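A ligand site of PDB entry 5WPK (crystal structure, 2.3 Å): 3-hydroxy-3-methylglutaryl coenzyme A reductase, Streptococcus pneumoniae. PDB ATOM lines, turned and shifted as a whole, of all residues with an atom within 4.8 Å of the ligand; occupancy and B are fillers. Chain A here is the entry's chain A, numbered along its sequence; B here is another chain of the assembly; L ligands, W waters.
The side-chain hydroxyl (OG) of Ser 85 lies within hydrogen-bond range of a nitrogen (N7) of the ligand, 2.9 Å away.
The guanidinium group (NH1) of Arg 259 is in salt-bridge range of an oxygen (O19) of the ligand.
An oxygen (O10) of the ligand lies close to the backbone carbonyl oxygen of Ser 91, 3.4 Å away.
N of Phe 10 is in hydrogen-bond range of O12 of the ligand, 3.1 Å away.
An oxygen (O12) of the ligand sits at hydrogen-bond distance from the side-chain hydroxyl (OG) of Ser 11 (3.0 Å).
N of Ser 11 sits at hydrogen-bond distance from O12 of the ligand, 2.8 Å away.
An oxygen (O11) of the ligand lies within salt-bridge range of the side-chain amino group of Lys 95 (3.2 Å).
The backbone NH (N) of Tyr 92 lies within hydrogen-bond range of an oxygen (O10) of the ligand.
A nitrogen (N7) of the ligand is in hydrogen-bond range of the backbone carbonyl oxygen (O) of Ser 85 (3.5 Å).
ND2 of Asn 269 is in hydrogen-bond range of O17 of the ligand, 2.8 Å away.
The side-chain sulfur (SD) of Met 381 sits at hydrogen-bond distance from a nitrogen (N5) of the ligand.
The backbone NH (N) of Gly 9 sits at hydrogen-bond distance from an oxygen (O11) of the ligand (3.1 Å).
N of Ser 85 sits at hydrogen-bond distance from OE2 of Glu 52 of chain B, 2.7 Å away.
The side-chain amide nitrogen of Asn 53 of chain B sits at hydrogen-bond distance from the side-chain hydroxyl of Ser 91 (3.1 Å).
NE2 of His 263 lies within hydrogen-bond range of OD1 of Asn 364.
OE1 of Glu 83 sits close to OD1 of Asn 269, 3.4 Å away.
The side-chain carboxylate of Glu 52 of chain B sits at hydrogen-bond distance from the backbone NH of Ala 88, 3.1 Å away.
The side-chain amide nitrogen (NE2) of Gln 363 lies within hydrogen-bond range of the backbone carbonyl oxygen (O) of Val 86, 2.9 Å away.
OE2 of Glu 83 lies close to S1 of the ligand.
Residues that only touch the ligand: Asn 53 of chain B, Leu 371, Thr 262, Ala 367, Glu 52 of chain B, Ala 88, Ala 89, Ile 376, Asn 8, Val 86, Trp 7, Ala 366, Gly 266, Ala 370, Ile 211 of chain B and His 263.
Hydrophobic or aromatic side chains that line the ligand: Val 86, Ala 88, Ala 89, Tyr 92, Ala 366, Ala 367, Ala 370, Leu 371, Ile 376, Met 381 and Ile 211 of chain B.
27 residues have an atom within 4 Å of the ligand: Trp 7, Asn 8, Gly 9, Phe 10, Ser 11, Glu 83, Ser 85, Val 86, Ala 88, Ala 89, Ser 91, Tyr 92, Lys 95, Arg 259, Thr 262, His 263, Gly 266, Asn 269, Ala 366, Ala 367, Ala 370, Leu 371, Ile 376, Met 381, Glu 52 of chain B, Asn 53 of chain B and Ile 211 of chain B.
The nearest printed residue that does not touch the ligand is Pro 84 (4.3 Å).
Water W4 bridges O5 of the ligand (2.4 Å) and OG of Ser 11 (2.5 Å).
Water W6 bridges an oxygen (O16) of the ligand and the side-chain amide nitrogen (NE2) of Gln 363.
Water W5 lies within hydrogen-bond range of O of Gly 266, O17 of the ligand and ND2 of Asn 269.
Water W12 lies within hydrogen-bond range of ND2 of Asn 53 of chain B (2.8 Å), N2 of the ligand (2.9 Å) and OG of Ser 91 (3.4 Å).
Water W2 lies within hydrogen-bond range of the backbone carbonyl oxygen of Ala 366 (2.8 Å) and an oxygen (O15) of the ligand (2.9 Å).
Water W11 lies within hydrogen-bond range of the backbone NH of Asn 53 of chain B (2.8 Å) and a nitrogen (N3) of the ligand (3.1 Å).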
ATOM      1  N   TRP A   7       6.401   0.360 -29.999  1.00  0.00           N
ATOM      2  CA  TRP A   7       7.735   0.291 -29.422  1.00  0.00           C
ATOM      3  C   TRP A   7       8.826   0.141 -30.468  1.00  0.00           C
ATOM      4  O   TRP A   7       9.951  -0.234 -30.126  1.00  0.00           O
ATOM      5  CB  TRP A   7       7.818  -0.863 -28.420  1.00  0.00           C
ATOM      6  CG  TRP A   7       6.973  -0.692 -27.191  1.00  0.00           C
ATOM      7  CD1 TRP A   7       5.702  -1.134 -26.999  1.00  0.00           C
ATOM      8  CD2 TRP A   7       7.365  -0.053 -25.965  1.00  0.00           C
ATOM      9  NE1 TRP A   7       5.272  -0.814 -25.744  1.00  0.00           N
ATOM     10  CE2 TRP A   7       6.279  -0.147 -25.082  1.00  0.00           C
ATOM     11  CE3 TRP A   7       8.538   0.576 -25.528  1.00  0.00           C
ATOM     12  CZ2 TRP A   7       6.307   0.376 -23.784  1.00  0.00           C
ATOM     13  CZ3 TRP A   7       8.570   1.101 -24.239  1.00  0.00           C
ATOM     14  CH2 TRP A   7       7.458   0.992 -23.395  1.00  0.00           C
ATOM     15  N   ASN A   8       8.528   0.406 -31.736  1.00  0.00           N
ATOM     16  CA  ASN A   8       9.533   0.239 -32.782  1.00  0.00           C
ATOM     17  C   ASN A   8      10.603   1.309 -32.670  1.00  0.00           C
ATOM     18  O   ASN A   8      10.312   2.482 -32.466  1.00  0.00           O
ATOM     19  CB  ASN A   8       8.879   0.289 -34.167  1.00  0.00           C
ATOM     20  CG  ASN A   8       8.138  -0.993 -34.500  1.00  0.00           C
ATOM     21  OD1 ASN A   8       8.491  -2.073 -34.017  1.00  0.00           O
ATOM     22  ND2 ASN A   8       7.098  -0.881 -35.328  1.00  0.00           N
ATOM     23  N   GLY A   9      11.866   0.884 -32.805  1.00  0.00           N
ATOM     24  CA  GLY A   9      12.967   1.793 -32.607  1.00  0.00           C
ATOM     25  C   GLY A   9      13.243   2.169 -31.168  1.00  0.00           C
ATOM     26  O   GLY A   9      14.001   3.110 -30.926  1.00  0.00           O
ATOM     27  N   PHE A  10      12.640   1.466 -30.209  1.00  0.00           N
ATOM     28  CA  PHE A  10      12.894   1.748 -28.793  1.00  0.00           C
ATOM     29  C   PHE A  10      14.355   1.501 -28.423  1.00  0.00           C
ATOM     30  O   PHE A  10      14.911   2.214 -27.589  1.00  0.00           O
ATOM     31  CB  PHE A  10      11.977   0.897 -27.932  1.00  0.00           C
ATOM     32  CG  PHE A  10      12.097   1.153 -26.452  1.00  0.00           C
ATOM     33  CD1 PHE A  10      11.846   2.408 -25.936  1.00  0.00           C
ATOM     34  CD2 PHE A  10      12.417   0.120 -25.585  1.00  0.00           C
ATOM     35  CE1 PHE A  10      11.930   2.640 -24.567  1.00  0.00           C
ATOM     36  CE2 PHE A  10      12.500   0.346 -24.229  1.00  0.00           C
ATOM     37  CZ  PHE A  10      12.266   1.603 -23.715  1.00  0.00           C
ATOM     38  N   SER A  11      14.976   0.484 -29.026  1.00  0.00           N
ATOM     39  CA  SER A  11      16.416   0.264 -28.866  1.00  0.00           C
ATOM     40  C   SER A  11      17.215   1.548 -29.078  1.00  0.00           C
ATOM     41  O   SER A  11      18.144   1.850 -28.322  1.00  0.00           O
ATOM     42  CB  SER A  11      16.903  -0.851 -29.798  1.00  0.00           C
ATOM     43  OG  SER A  11      16.915  -0.425 -31.148  1.00  0.00           O
ATOM     44  N   LYS A  12      16.868   2.312 -30.117  1.00  0.00           N
ATOM     45  CA  LYS A  12      17.666   3.468 -30.526  1.00  0.00           C
ATOM     46  C   LYS A  12      17.334   4.731 -29.745  1.00  0.00           C
ATOM     47  O   LYS A  12      17.923   5.777 -30.026  1.00  0.00           O
ATOM     48  CB  LYS A  12      17.466   3.731 -32.015  1.00  0.00           C
ATOM     49  CG  LYS A  12      17.488   2.492 -32.893  1.00  0.00           C
ATOM     50  CD  LYS A  12      18.896   1.972 -33.080  1.00  0.00           C
ATOM     51  CE  LYS A  12      18.910   0.755 -33.993  1.00  0.00           C
ATOM     52  NZ  LYS A  12      18.205   1.021 -35.275  1.00  0.00           N
ATOM     53  N   GLU A  83      24.197  -7.187 -16.571  1.00  0.00           N
ATOM     54  CA  GLU A  83      24.921  -7.852 -17.653  1.00  0.00           C
ATOM     55  C   GLU A  83      24.485  -7.311 -19.001  1.00  0.00           C
ATOM     56  O   GLU A  83      23.283  -7.360 -19.323  1.00  0.00           O
ATOM     57  CB  GLU A  83      24.701  -9.356 -17.593  1.00  0.00           C
ATOM     58  CG  GLU A  83      25.416 -10.090 -18.711  1.00  0.00           C
ATOM     59  CD  GLU A  83      25.240 -11.584 -18.627  1.00  0.00           C
ATOM     60  OE1 GLU A  83      24.637 -12.062 -17.639  1.00  0.00           O
ATOM     61  OE2 GLU A  83      25.724 -12.294 -19.532  1.00  0.00           O
ATOM     62  N   PRO A  84      25.403  -6.805 -19.815  1.00  0.00           N
ATOM     63  CA  PRO A  84      25.028  -6.315 -21.150  1.00  0.00           C
ATOM     64  C   PRO A  84      24.419  -7.416 -22.014  1.00  0.00           C
ATOM     65  O   PRO A  84      24.753  -8.602 -21.882  1.00  0.00           O
ATOM     66  CB  PRO A  84      26.355  -5.824 -21.736  1.00  0.00           C
ATOM     67  CG  PRO A  84      27.210  -5.525 -20.544  1.00  0.00           C
ATOM     68  CD  PRO A  84      26.818  -6.532 -19.505  1.00  0.00           C
ATOM     69  N   SER A  85      23.521  -6.999 -22.913  1.00  0.00           N
ATOM     70  CA  SER A  85      22.823  -7.772 -23.927  1.00  0.00           C
ATOM     71  C   SER A  85      21.689  -8.605 -23.343  1.00  0.00           C
ATOM     72  O   SER A  85      20.919  -9.188 -24.122  1.00  0.00           O
ATOM     73  CB  SER A  85      23.748  -8.713 -24.728  1.00  0.00           C
ATOM     74  OG  SER A  85      24.154  -9.824 -23.940  1.00  0.00           O
ATOM     75  N   VAL A  86      21.552  -8.707 -22.027  1.00  0.00           N
ATOM     76  CA  VAL A  86      20.468  -9.492 -21.456  1.00  0.00           C
ATOM     77  C   VAL A  86      19.115  -8.871 -21.792  1.00  0.00           C
ATOM     78  O   VAL A  86      18.204  -9.547 -22.282  1.00  0.00           O
ATOM     79  CB  VAL A  86      20.653  -9.637 -19.937  1.00  0.00           C
ATOM     80  CG1 VAL A  86      19.386 -10.156 -19.279  1.00  0.00           C
ATOM     81  CG2 VAL A  86      21.832 -10.560 -19.625  1.00  0.00           C
ATOM     82  N   ALA A  88      18.511  -6.551 -24.140  1.00  0.00           N
ATOM     83  CA  ALA A  88      18.345  -6.523 -25.586  1.00  0.00           C
ATOM     84  C   ALA A  88      17.886  -7.866 -26.134  1.00  0.00           C
ATOM     85  O   ALA A  88      17.044  -7.921 -27.029  1.00  0.00           O
ATOM     86  CB  ALA A  88      19.657  -6.099 -26.256  1.00  0.00           C
ATOM     87  N   ALA A  89      18.414  -8.961 -25.587  1.00  0.00           N
ATOM     88  CA  ALA A  89      18.054 -10.283 -26.082  1.00  0.00           C
ATOM     89  C   ALA A  89      16.624 -10.649 -25.702  1.00  0.00           C
ATOM     90  O   ALA A  89      15.894 -11.247 -26.507  1.00  0.00           O
ATOM     91  CB  ALA A  89      19.027 -11.336 -25.553  1.00  0.00           C
ATOM     92  N   SER A  91      14.203  -8.480 -25.166  1.00  0.00           N
ATOM     93  CA  SER A  91      13.331  -7.632 -25.973  1.00  0.00           C
ATOM     94  C   SER A  91      13.224  -8.170 -27.393  1.00  0.00           C
ATOM     95  O   SER A  91      12.130  -8.239 -27.967  1.00  0.00           O
ATOM     96  CB  SER A  91      13.853  -6.199 -25.991  1.00  0.00           C
ATOM     97  OG  SER A  91      13.923  -5.672 -24.683  1.00  0.00           O
ATOM     98  N   TYR A  92      14.360  -8.555 -27.983  1.00  0.00           N
ATOM     99  CA  TYR A  92      14.376  -9.112 -29.330  1.00  0.00           C
ATOM    100  C   TYR A  92      13.552 -10.393 -29.412  1.00  0.00           C
ATOM    101  O   TYR A  92      12.750 -10.570 -30.337  1.00  0.00           O
ATOM    102  CB  TYR A  92      15.818  -9.362 -29.760  1.00  0.00           C
ATOM    103  CG  TYR A  92      15.977 -10.063 -31.087  1.00  0.00           C
ATOM    104  CD1 TYR A  92      16.240 -11.420 -31.147  1.00  0.00           C
ATOM    105  CD2 TYR A  92      15.879  -9.354 -32.277  1.00  0.00           C
ATOM    106  CE1 TYR A  92      16.391 -12.066 -32.359  1.00  0.00           C
ATOM    107  CE2 TYR A  92      16.033  -9.984 -33.496  1.00  0.00           C
ATOM    108  CZ  TYR A  92      16.292 -11.337 -33.535  1.00  0.00           C
ATOM    109  OH  TYR A  92      16.444 -11.982 -34.747  1.00  0.00           O
ATOM    110  N   LYS A  95       9.728  -9.723 -29.166  1.00  0.00           N
ATOM    111  CA  LYS A  95       9.124  -9.161 -30.360  1.00  0.00           C
ATOM    112  C   LYS A  95       8.831 -10.252 -31.390  1.00  0.00           C
ATOM    113  O   LYS A  95       7.738 -10.292 -31.971  1.00  0.00           O
ATOM    114  CB  LYS A  95      10.029  -8.094 -30.963  1.00  0.00           C
ATOM    115  CG  LYS A  95       9.299  -7.096 -31.850  1.00  0.00           C
ATOM    116  CD  LYS A  95      10.237  -6.432 -32.848  1.00  0.00           C
ATOM    117  CE  LYS A  95      11.457  -5.844 -32.156  1.00  0.00           C
ATOM    118  NZ  LYS A  95      11.063  -4.888 -31.074  1.00  0.00           N
ATOM    119  N   ARG A 259      26.597 -28.451 -20.807  1.00  0.00           N
ATOM    120  CA  ARG A 259      25.768 -27.529 -21.584  1.00  0.00           C
ATOM    121  C   ARG A 259      24.516 -27.127 -20.803  1.00  0.00           C
ATOM    122  O   ARG A 259      24.116 -25.956 -20.835  1.00  0.00           O
ATOM    123  CB  ARG A 259      25.374 -28.168 -22.913  1.00  0.00           C
ATOM    124  CG  ARG A 259      24.430 -27.332 -23.748  1.00  0.00           C
ATOM    125  CD  ARG A 259      24.948 -25.930 -23.941  1.00  0.00           C
ATOM    126  NE  ARG A 259      23.882 -25.032 -24.345  1.00  0.00           N
ATOM    127  CZ  ARG A 259      23.929 -23.701 -24.233  1.00  0.00           C
ATOM    128  NH1 ARG A 259      25.003 -23.131 -23.719  1.00  0.00           N
ATOM    129  NH2 ARG A 259      22.901 -22.971 -24.627  1.00  0.00           N
ATOM    130  N   THR A 262      24.971 -24.006 -18.601  1.00  0.00           N
ATOM    131  CA  THR A 262      24.961 -22.757 -19.340  1.00  0.00           C
ATOM    132  C   THR A 262      23.578 -22.465 -19.913  1.00  0.00           C
ATOM    133  O   THR A 262      23.100 -21.323 -19.853  1.00  0.00           O
ATOM    134  CB  THR A 262      25.982 -22.822 -20.478  1.00  0.00           C
ATOM    135  OG1 THR A 262      27.128 -23.564 -20.048  1.00  0.00           O
ATOM    136  CG2 THR A 262      26.416 -21.420 -20.894  1.00  0.00           C
ATOM    137  N   HIS A 263      22.937 -23.491 -20.479  1.00  0.00           N
ATOM    138  CA  HIS A 263      21.576 -23.365 -20.994  1.00  0.00           C
ATOM    139  C   HIS A 263      20.645 -22.807 -19.929  1.00  0.00           C
ATOM    140  O   HIS A 263      19.928 -21.833 -20.170  1.00  0.00           O
ATOM    141  CB  HIS A 263      21.120 -24.750 -21.467  1.00  0.00           C
ATOM    142  CG  HIS A 263      19.710 -24.794 -21.972  1.00  0.00           C
ATOM    143  ND1 HIS A 263      19.393 -24.853 -23.313  1.00  0.00           N
ATOM    144  CD2 HIS A 263      18.523 -24.826 -21.303  1.00  0.00           C
ATOM    145  CE1 HIS A 263      18.083 -24.912 -23.453  1.00  0.00           C
ATOM    146  NE2 HIS A 263      17.534 -24.893 -22.251  1.00  0.00           N
ATOM    147  N   GLY A 266      21.458 -19.040 -18.852  1.00  0.00           N
ATOM    148  CA  GLY A 266      20.845 -18.039 -19.701  1.00  0.00           C
ATOM    149  C   GLY A 266      19.375 -17.819 -19.414  1.00  0.00           C
ATOM    150  O   GLY A 266      18.868 -16.709 -19.542  1.00  0.00           O
ATOM    151  N   ASN A 269      19.222 -15.471 -16.376  1.00  0.00           N
ATOM    152  CA  ASN A 269      19.602 -14.081 -16.607  1.00  0.00           C
ATOM    153  C   ASN A 269      18.356 -13.204 -16.676  1.00  0.00           C
ATOM    154  O   ASN A 269      18.336 -12.090 -16.140  1.00  0.00           O
ATOM    155  CB  ASN A 269      20.414 -13.944 -17.893  1.00  0.00           C
ATOM    156  CG  ASN A 269      21.861 -14.364 -17.721  1.00  0.00           C
ATOM    157  OD1 ASN A 269      22.366 -14.426 -16.605  1.00  0.00           O
ATOM    158  ND2 ASN A 269      22.530 -14.641 -18.827  1.00  0.00           N
ATOM    159  N   GLN A 363      14.059 -15.401 -22.917  1.00  0.00           N
ATOM    160  CA  GLN A 363      15.496 -15.238 -22.744  1.00  0.00           C
ATOM    161  C   GLN A 363      16.254 -16.451 -23.292  1.00  0.00           C
ATOM    162  O   GLN A 363      17.258 -16.293 -23.993  1.00  0.00           O
ATOM    163  CB  GLN A 363      15.838 -15.021 -21.270  1.00  0.00           C
ATOM    164  CG  GLN A 363      17.212 -14.419 -21.051  1.00  0.00           C
ATOM    165  CD  GLN A 363      17.224 -12.927 -21.263  1.00  0.00           C
ATOM    166  OE1 GLN A 363      16.571 -12.179 -20.530  1.00  0.00           O
ATOM    167  NE2 GLN A 363      17.956 -12.470 -22.267  1.00  0.00           N
ATOM    168  N   ASN A 364      15.776 -17.657 -22.986  1.00  0.00           N
ATOM    169  CA  ASN A 364      16.432 -18.855 -23.493  1.00  0.00           C
ATOM    170  C   ASN A 364      16.414 -18.884 -25.017  1.00  0.00           C
ATOM    171  O   ASN A 364      17.396 -19.297 -25.644  1.00  0.00           O
ATOM    172  CB  ASN A 364      15.768 -20.102 -22.914  1.00  0.00           C
ATOM    173  CG  ASN A 364      16.444 -21.388 -23.354  1.00  0.00           C
ATOM    174  OD1 ASN A 364      15.787 -22.341 -23.773  1.00  0.00           O
ATOM    175  ND2 ASN A 364      17.763 -21.417 -23.266  1.00  0.00           N
ATOM    176  N   ALA A 366      16.416 -16.338 -27.211  1.00  0.00           N
ATOM    177  CA  ALA A 366      17.349 -15.411 -27.817  1.00  0.00           C
ATOM    178  C   ALA A 366      18.784 -15.920 -27.719  1.00  0.00           C
ATOM    179  O   ALA A 366      19.587 -15.718 -28.640  1.00  0.00           O
ATOM    180  CB  ALA A 366      17.227 -14.037 -27.165  1.00  0.00           C
ATOM    181  N   ALA A 367      19.130 -16.582 -26.612  1.00  0.00           N
ATOM    182  CA  ALA A 367      20.472 -17.140 -26.465  1.00  0.00           C
ATOM    183  C   ALA A 367      20.716 -18.246 -27.485  1.00  0.00           C
ATOM    184  O   ALA A 367      21.735 -18.251 -28.177  1.00  0.00           O
ATOM    185  CB  ALA A 367      20.662 -17.656 -25.047  1.00  0.00           C
ATOM    186  N   LEU A 368      19.781 -19.195 -27.581  1.00  0.00           N
ATOM    187  CA  LEU A 368      19.954 -20.322 -28.504  1.00  0.00           C
ATOM    188  C   LEU A 368      20.017 -19.849 -29.946  1.00  0.00           C
ATOM    189  O   LEU A 368      20.806 -20.370 -30.740  1.00  0.00           O
ATOM    190  CB  LEU A 368      18.824 -21.333 -28.323  1.00  0.00           C
ATOM    191  CG  LEU A 368      18.639 -21.944 -26.937  1.00  0.00           C
ATOM    192  CD1 LEU A 368      17.599 -23.050 -26.994  1.00  0.00           C
ATOM    193  CD2 LEU A 368      19.961 -22.474 -26.414  1.00  0.00           C
ATOM    194  N   ALA A 370      21.182 -17.076 -31.072  1.00  0.00           N
ATOM    195  CA  ALA A 370      22.473 -16.448 -31.343  1.00  0.00           C
ATOM    196  C   ALA A 370      23.610 -17.467 -31.336  1.00  0.00           C
ATOM    197  O   ALA A 370      24.443 -17.455 -32.243  1.00  0.00           O
ATOM    198  CB  ALA A 370      22.735 -15.345 -30.316  1.00  0.00           C
ATOM    199  N   LEU A 371      23.644 -18.375 -30.350  1.00  0.00           N
ATOM    200  CA  LEU A 371      24.727 -19.342 -30.262  1.00  0.00           C
ATOM    201  C   LEU A 371      24.803 -20.192 -31.515  1.00  0.00           C
ATOM    202  O   LEU A 371      25.894 -20.601 -31.938  1.00  0.00           O
ATOM    203  CB  LEU A 371      24.542 -20.248 -29.037  1.00  0.00           C
ATOM    204  CG  LEU A 371      24.733 -19.560 -27.692  1.00  0.00           C
ATOM    205  CD1 LEU A 371      24.214 -20.444 -26.577  1.00  0.00           C
ATOM    206  CD2 LEU A 371      26.191 -19.246 -27.501  1.00  0.00           C
ATOM    207  N   ILE A 376      27.866 -15.824 -29.877  1.00  0.00           N
ATOM    208  CA  ILE A 376      28.043 -14.778 -28.877  1.00  0.00           C
ATOM    209  C   ILE A 376      29.531 -14.564 -28.639  1.00  0.00           C
ATOM    210  O   ILE A 376      30.101 -15.127 -27.688  1.00  0.00           O
ATOM    211  CB  ILE A 376      27.292 -15.116 -27.574  1.00  0.00           C
ATOM    212  CG1 ILE A 376      25.854 -15.511 -27.901  1.00  0.00           C
ATOM    213  CG2 ILE A 376      27.322 -13.926 -26.620  1.00  0.00           C
ATOM    214  CD1 ILE A 376      24.872 -15.327 -26.762  1.00  0.00           C
ATOM    215  N   MET A 381      27.898  -3.222 -27.688  1.00  0.00           N
ATOM    216  CA  MET A 381      27.170  -2.155 -28.340  1.00  0.00           C
ATOM    217  C   MET A 381      27.654  -0.781 -27.888  1.00  0.00           C
ATOM    218  O   MET A 381      28.204  -0.017 -28.675  1.00  0.00           O
ATOM    219  CB  MET A 381      25.674  -2.335 -28.071  1.00  0.00           C
ATOM    220  CG  MET A 381      25.408  -3.002 -26.722  1.00  0.00           C
ATOM    221  SD  MET A 381      23.812  -3.830 -26.619  1.00  0.00           S
ATOM    222  CE  MET A 381      24.029  -5.155 -27.803  1.00  0.00           C
ATOM    223  N   GLU B  52      20.531  -2.435 -21.337  1.00  0.00           N
ATOM    224  CA  GLU B  52      19.773  -1.840 -22.424  1.00  0.00           C
ATOM    225  C   GLU B  52      18.408  -1.396 -21.908  1.00  0.00           C
ATOM    226  O   GLU B  52      17.973  -1.797 -20.837  1.00  0.00           O
ATOM    227  CB  GLU B  52      19.614  -2.829 -23.588  1.00  0.00           C
ATOM    228  CG  GLU B  52      20.930  -3.354 -24.138  1.00  0.00           C
ATOM    229  CD  GLU B  52      21.585  -4.396 -23.238  1.00  0.00           C
ATOM    230  OE1 GLU B  52      20.861  -5.235 -22.662  1.00  0.00           O
ATOM    231  OE2 GLU B  52      22.830  -4.373 -23.090  1.00  0.00           O
ATOM    232  N   ASN B  53      17.745  -0.548 -22.701  1.00  0.00           N
ATOM    233  CA  ASN B  53      16.464   0.045 -22.339  1.00  0.00           C
ATOM    234  C   ASN B  53      16.429   0.530 -20.897  1.00  0.00           C
ATOM    235  O   ASN B  53      15.421   0.350 -20.201  1.00  0.00           O
ATOM    236  CB  ASN B  53      15.292  -0.935 -22.559  1.00  0.00           C
ATOM    237  CG  ASN B  53      15.295  -1.564 -23.934  1.00  0.00           C
ATOM    238  OD1 ASN B  53      15.732  -0.955 -24.911  1.00  0.00           O
ATOM    239  ND2 ASN B  53      14.729  -2.758 -24.032  1.00  0.00           N
ATOM    240  N   ILE B 211      30.762 -22.560 -26.947  1.00  0.00           N
ATOM    241  CA  ILE B 211      30.348 -21.706 -25.842  1.00  0.00           C
ATOM    242  C   ILE B 211      31.039 -22.152 -24.555  1.00  0.00           C
ATOM    243  O   ILE B 211      31.341 -23.325 -24.347  1.00  0.00           O
ATOM    244  CB  ILE B 211      28.807 -21.734 -25.678  1.00  0.00           C
ATOM    245  CG1 ILE B 211      28.352 -20.686 -24.660  1.00  0.00           C
ATOM    246  CG2 ILE B 211      28.325 -23.125 -25.296  1.00  0.00           C
ATOM    247  CD1 ILE B 211      28.758 -19.270 -25.009  1.00  0.00           C
HETATM  248  P1  LIG L   1      20.491  -7.635 -33.933  1.00  0.00           P
HETATM  249  O1  LIG L   1      21.691  -7.130 -34.706  1.00  0.00           O
HETATM  250  O2  LIG L   1      19.543  -8.362 -34.854  1.00  0.00           O
HETATM  251  O3  LIG L   1      19.721  -6.364 -33.215  1.00  0.00           O
HETATM  252  O4  LIG L   1      21.006  -8.648 -32.751  1.00  0.00           O
HETATM  253  P2  LIG L   1      18.723  -5.310 -34.005  1.00  0.00           P
HETATM  254  O5  LIG L   1      19.043  -3.896 -33.552  1.00  0.00           O
HETATM  255  O6  LIG L   1      18.924  -5.410 -35.495  1.00  0.00           O
HETATM  256  O7  LIG L   1      17.173  -5.696 -33.620  1.00  0.00           O
HETATM  257  C1  LIG L   1      16.370  -4.702 -33.078  1.00  0.00           C
HETATM  258  C2  LIG L   1      15.458  -5.313 -31.982  1.00  0.00           C
HETATM  259  O8  LIG L   1      16.107  -6.199 -31.280  1.00  0.00           O
HETATM  260  C3  LIG L   1      15.042  -4.194 -31.003  1.00  0.00           C
HETATM  261  O9  LIG L   1      13.779  -3.792 -31.253  1.00  0.00           O
HETATM  262  C4  LIG L   1      15.128  -4.868 -29.623  1.00  0.00           C
HETATM  263  O10 LIG L   1      13.877  -5.636 -29.348  1.00  0.00           O
HETATM  264  C5  LIG L   1      16.146  -5.685 -29.740  1.00  0.00           C
HETATM  265  P3  LIG L   1      13.544  -2.324 -31.988  1.00  0.00           P
HETATM  266  O11 LIG L   1      12.069  -2.149 -32.272  1.00  0.00           O
HETATM  267  O12 LIG L   1      14.005  -1.229 -31.052  1.00  0.00           O
HETATM  268  O13 LIG L   1      14.324  -2.269 -33.278  1.00  0.00           O
HETATM  269  N1  LIG L   1      17.382  -4.980 -29.466  1.00  0.00           N
HETATM  270  C6  LIG L   1      17.769  -4.100 -28.527  1.00  0.00           C
HETATM  271  N2  LIG L   1      17.126  -3.560 -27.477  1.00  0.00           N
HETATM  272  C7  LIG L   1      17.764  -2.679 -26.670  1.00  0.00           C
HETATM  273  N3  LIG L   1      19.060  -2.352 -26.910  1.00  0.00           N
HETATM  274  C8  LIG L   1      19.699  -2.887 -27.939  1.00  0.00           C
HETATM  275  C9  LIG L   1      19.042  -3.782 -28.768  1.00  0.00           C
HETATM  276  N4  LIG L   1      19.443  -4.460 -29.857  1.00  0.00           N
HETATM  277  C10 LIG L   1      18.412  -5.195 -30.291  1.00  0.00           C
HETATM  278  N5  LIG L   1      21.052  -2.374 -27.990  1.00  0.00           N
HETATM  279  C11 LIG L   1      20.747  -8.972 -30.408  1.00  0.00           C
HETATM  280  C12 LIG L   1      21.351  -8.100 -31.515  1.00  0.00           C
HETATM  281  C13 LIG L   1      21.474  -8.701 -29.103  1.00  0.00           C
HETATM  282  C14 LIG L   1      19.281  -8.605 -30.258  1.00  0.00           C
HETATM  283  C15 LIG L   1      20.885 -10.439 -30.816  1.00  0.00           C
HETATM  284  O14 LIG L   1      22.165 -10.671 -31.336  1.00  0.00           O
HETATM  285  C16 LIG L   1      20.663 -11.368 -29.624  1.00  0.00           C
HETATM  286  O15 LIG L   1      19.565 -11.612 -29.252  1.00  0.00           O
HETATM  287  N6  LIG L   1      21.813 -11.962 -28.958  1.00  0.00           N
HETATM  288  C17 LIG L   1      21.631 -12.840 -27.819  1.00  0.00           C
HETATM  289  C18 LIG L   1      22.603 -12.414 -26.732  1.00  0.00           C
HETATM  290  C19 LIG L   1      22.144 -12.918 -25.370  1.00  0.00           C
HETATM  291  O16 LIG L   1      21.421 -13.850 -25.278  1.00  0.00           O
HETATM  292  N7  LIG L   1      22.620 -12.232 -24.174  1.00  0.00           N
HETATM  293  C20 LIG L   1      22.225 -12.682 -22.852  1.00  0.00           C
HETATM  294  C21 LIG L   1      23.471 -12.690 -21.974  1.00  0.00           C
HETATM  295  S1  LIG L   1      24.635 -13.956 -22.559  1.00  0.00           S
HETATM  296  C22 LIG L   1      24.141 -15.539 -21.801  1.00  0.00           C
HETATM  297  O17 LIG L   1      23.042 -15.652 -21.368  1.00  0.00           O
HETATM  298  C23 LIG L   1      25.128 -16.703 -21.685  1.00  0.00           C
HETATM  299  C24 LIG L   1      24.744 -17.871 -22.590  1.00  0.00           C
HETATM  300  O18 LIG L   1      25.852 -18.702 -22.755  1.00  0.00           O
HETATM  301  C25 LIG L   1      23.596 -18.685 -21.999  1.00  0.00           C
HETATM  302  C26 LIG L   1      23.274 -19.858 -22.930  1.00  0.00           C
HETATM  303  O19 LIG L   1      24.210 -20.566 -23.381  1.00  0.00           O
HETATM  304  O20 LIG L   1      22.081 -20.121 -23.240  1.00  0.00           O
HETATM  305  C27 LIG L   1      24.307 -17.335 -23.951  1.00  0.00           C
HETATM  306  O   HOH W   1      16.499  -8.439 -36.360  1.00  0.00           O
HETATM  307  O   HOH W   2      18.812 -14.023 -30.771  1.00  0.00           O
HETATM  308  O   HOH W   3      22.122 -12.029 -33.649  1.00  0.00           O
HETATM  309  O   HOH W   4      18.561  -1.923 -32.251  1.00  0.00           O
HETATM  310  O   HOH W   5      20.322 -15.074 -20.778  1.00  0.00           O
HETATM  311  O   HOH W   6      19.513 -14.451 -23.533  1.00  0.00           O
HETATM  312  O   HOH W   7      24.037  -9.968 -34.168  1.00  0.00           O
HETATM  313  O   HOH W   8      19.821 -20.098 -22.058  1.00  0.00           O
HETATM  314  O   HOH W   9      25.234 -12.208 -31.250  1.00  0.00           O
HETATM  315  O   HOH W  10      18.744 -11.034 -35.380  1.00  0.00           O
HETATM  316  O   HOH W  11      19.019   0.128 -25.051  1.00  0.00           O
HETATM  317  O   HOH W  12      14.336  -3.037 -26.804  1.00  0.00           O
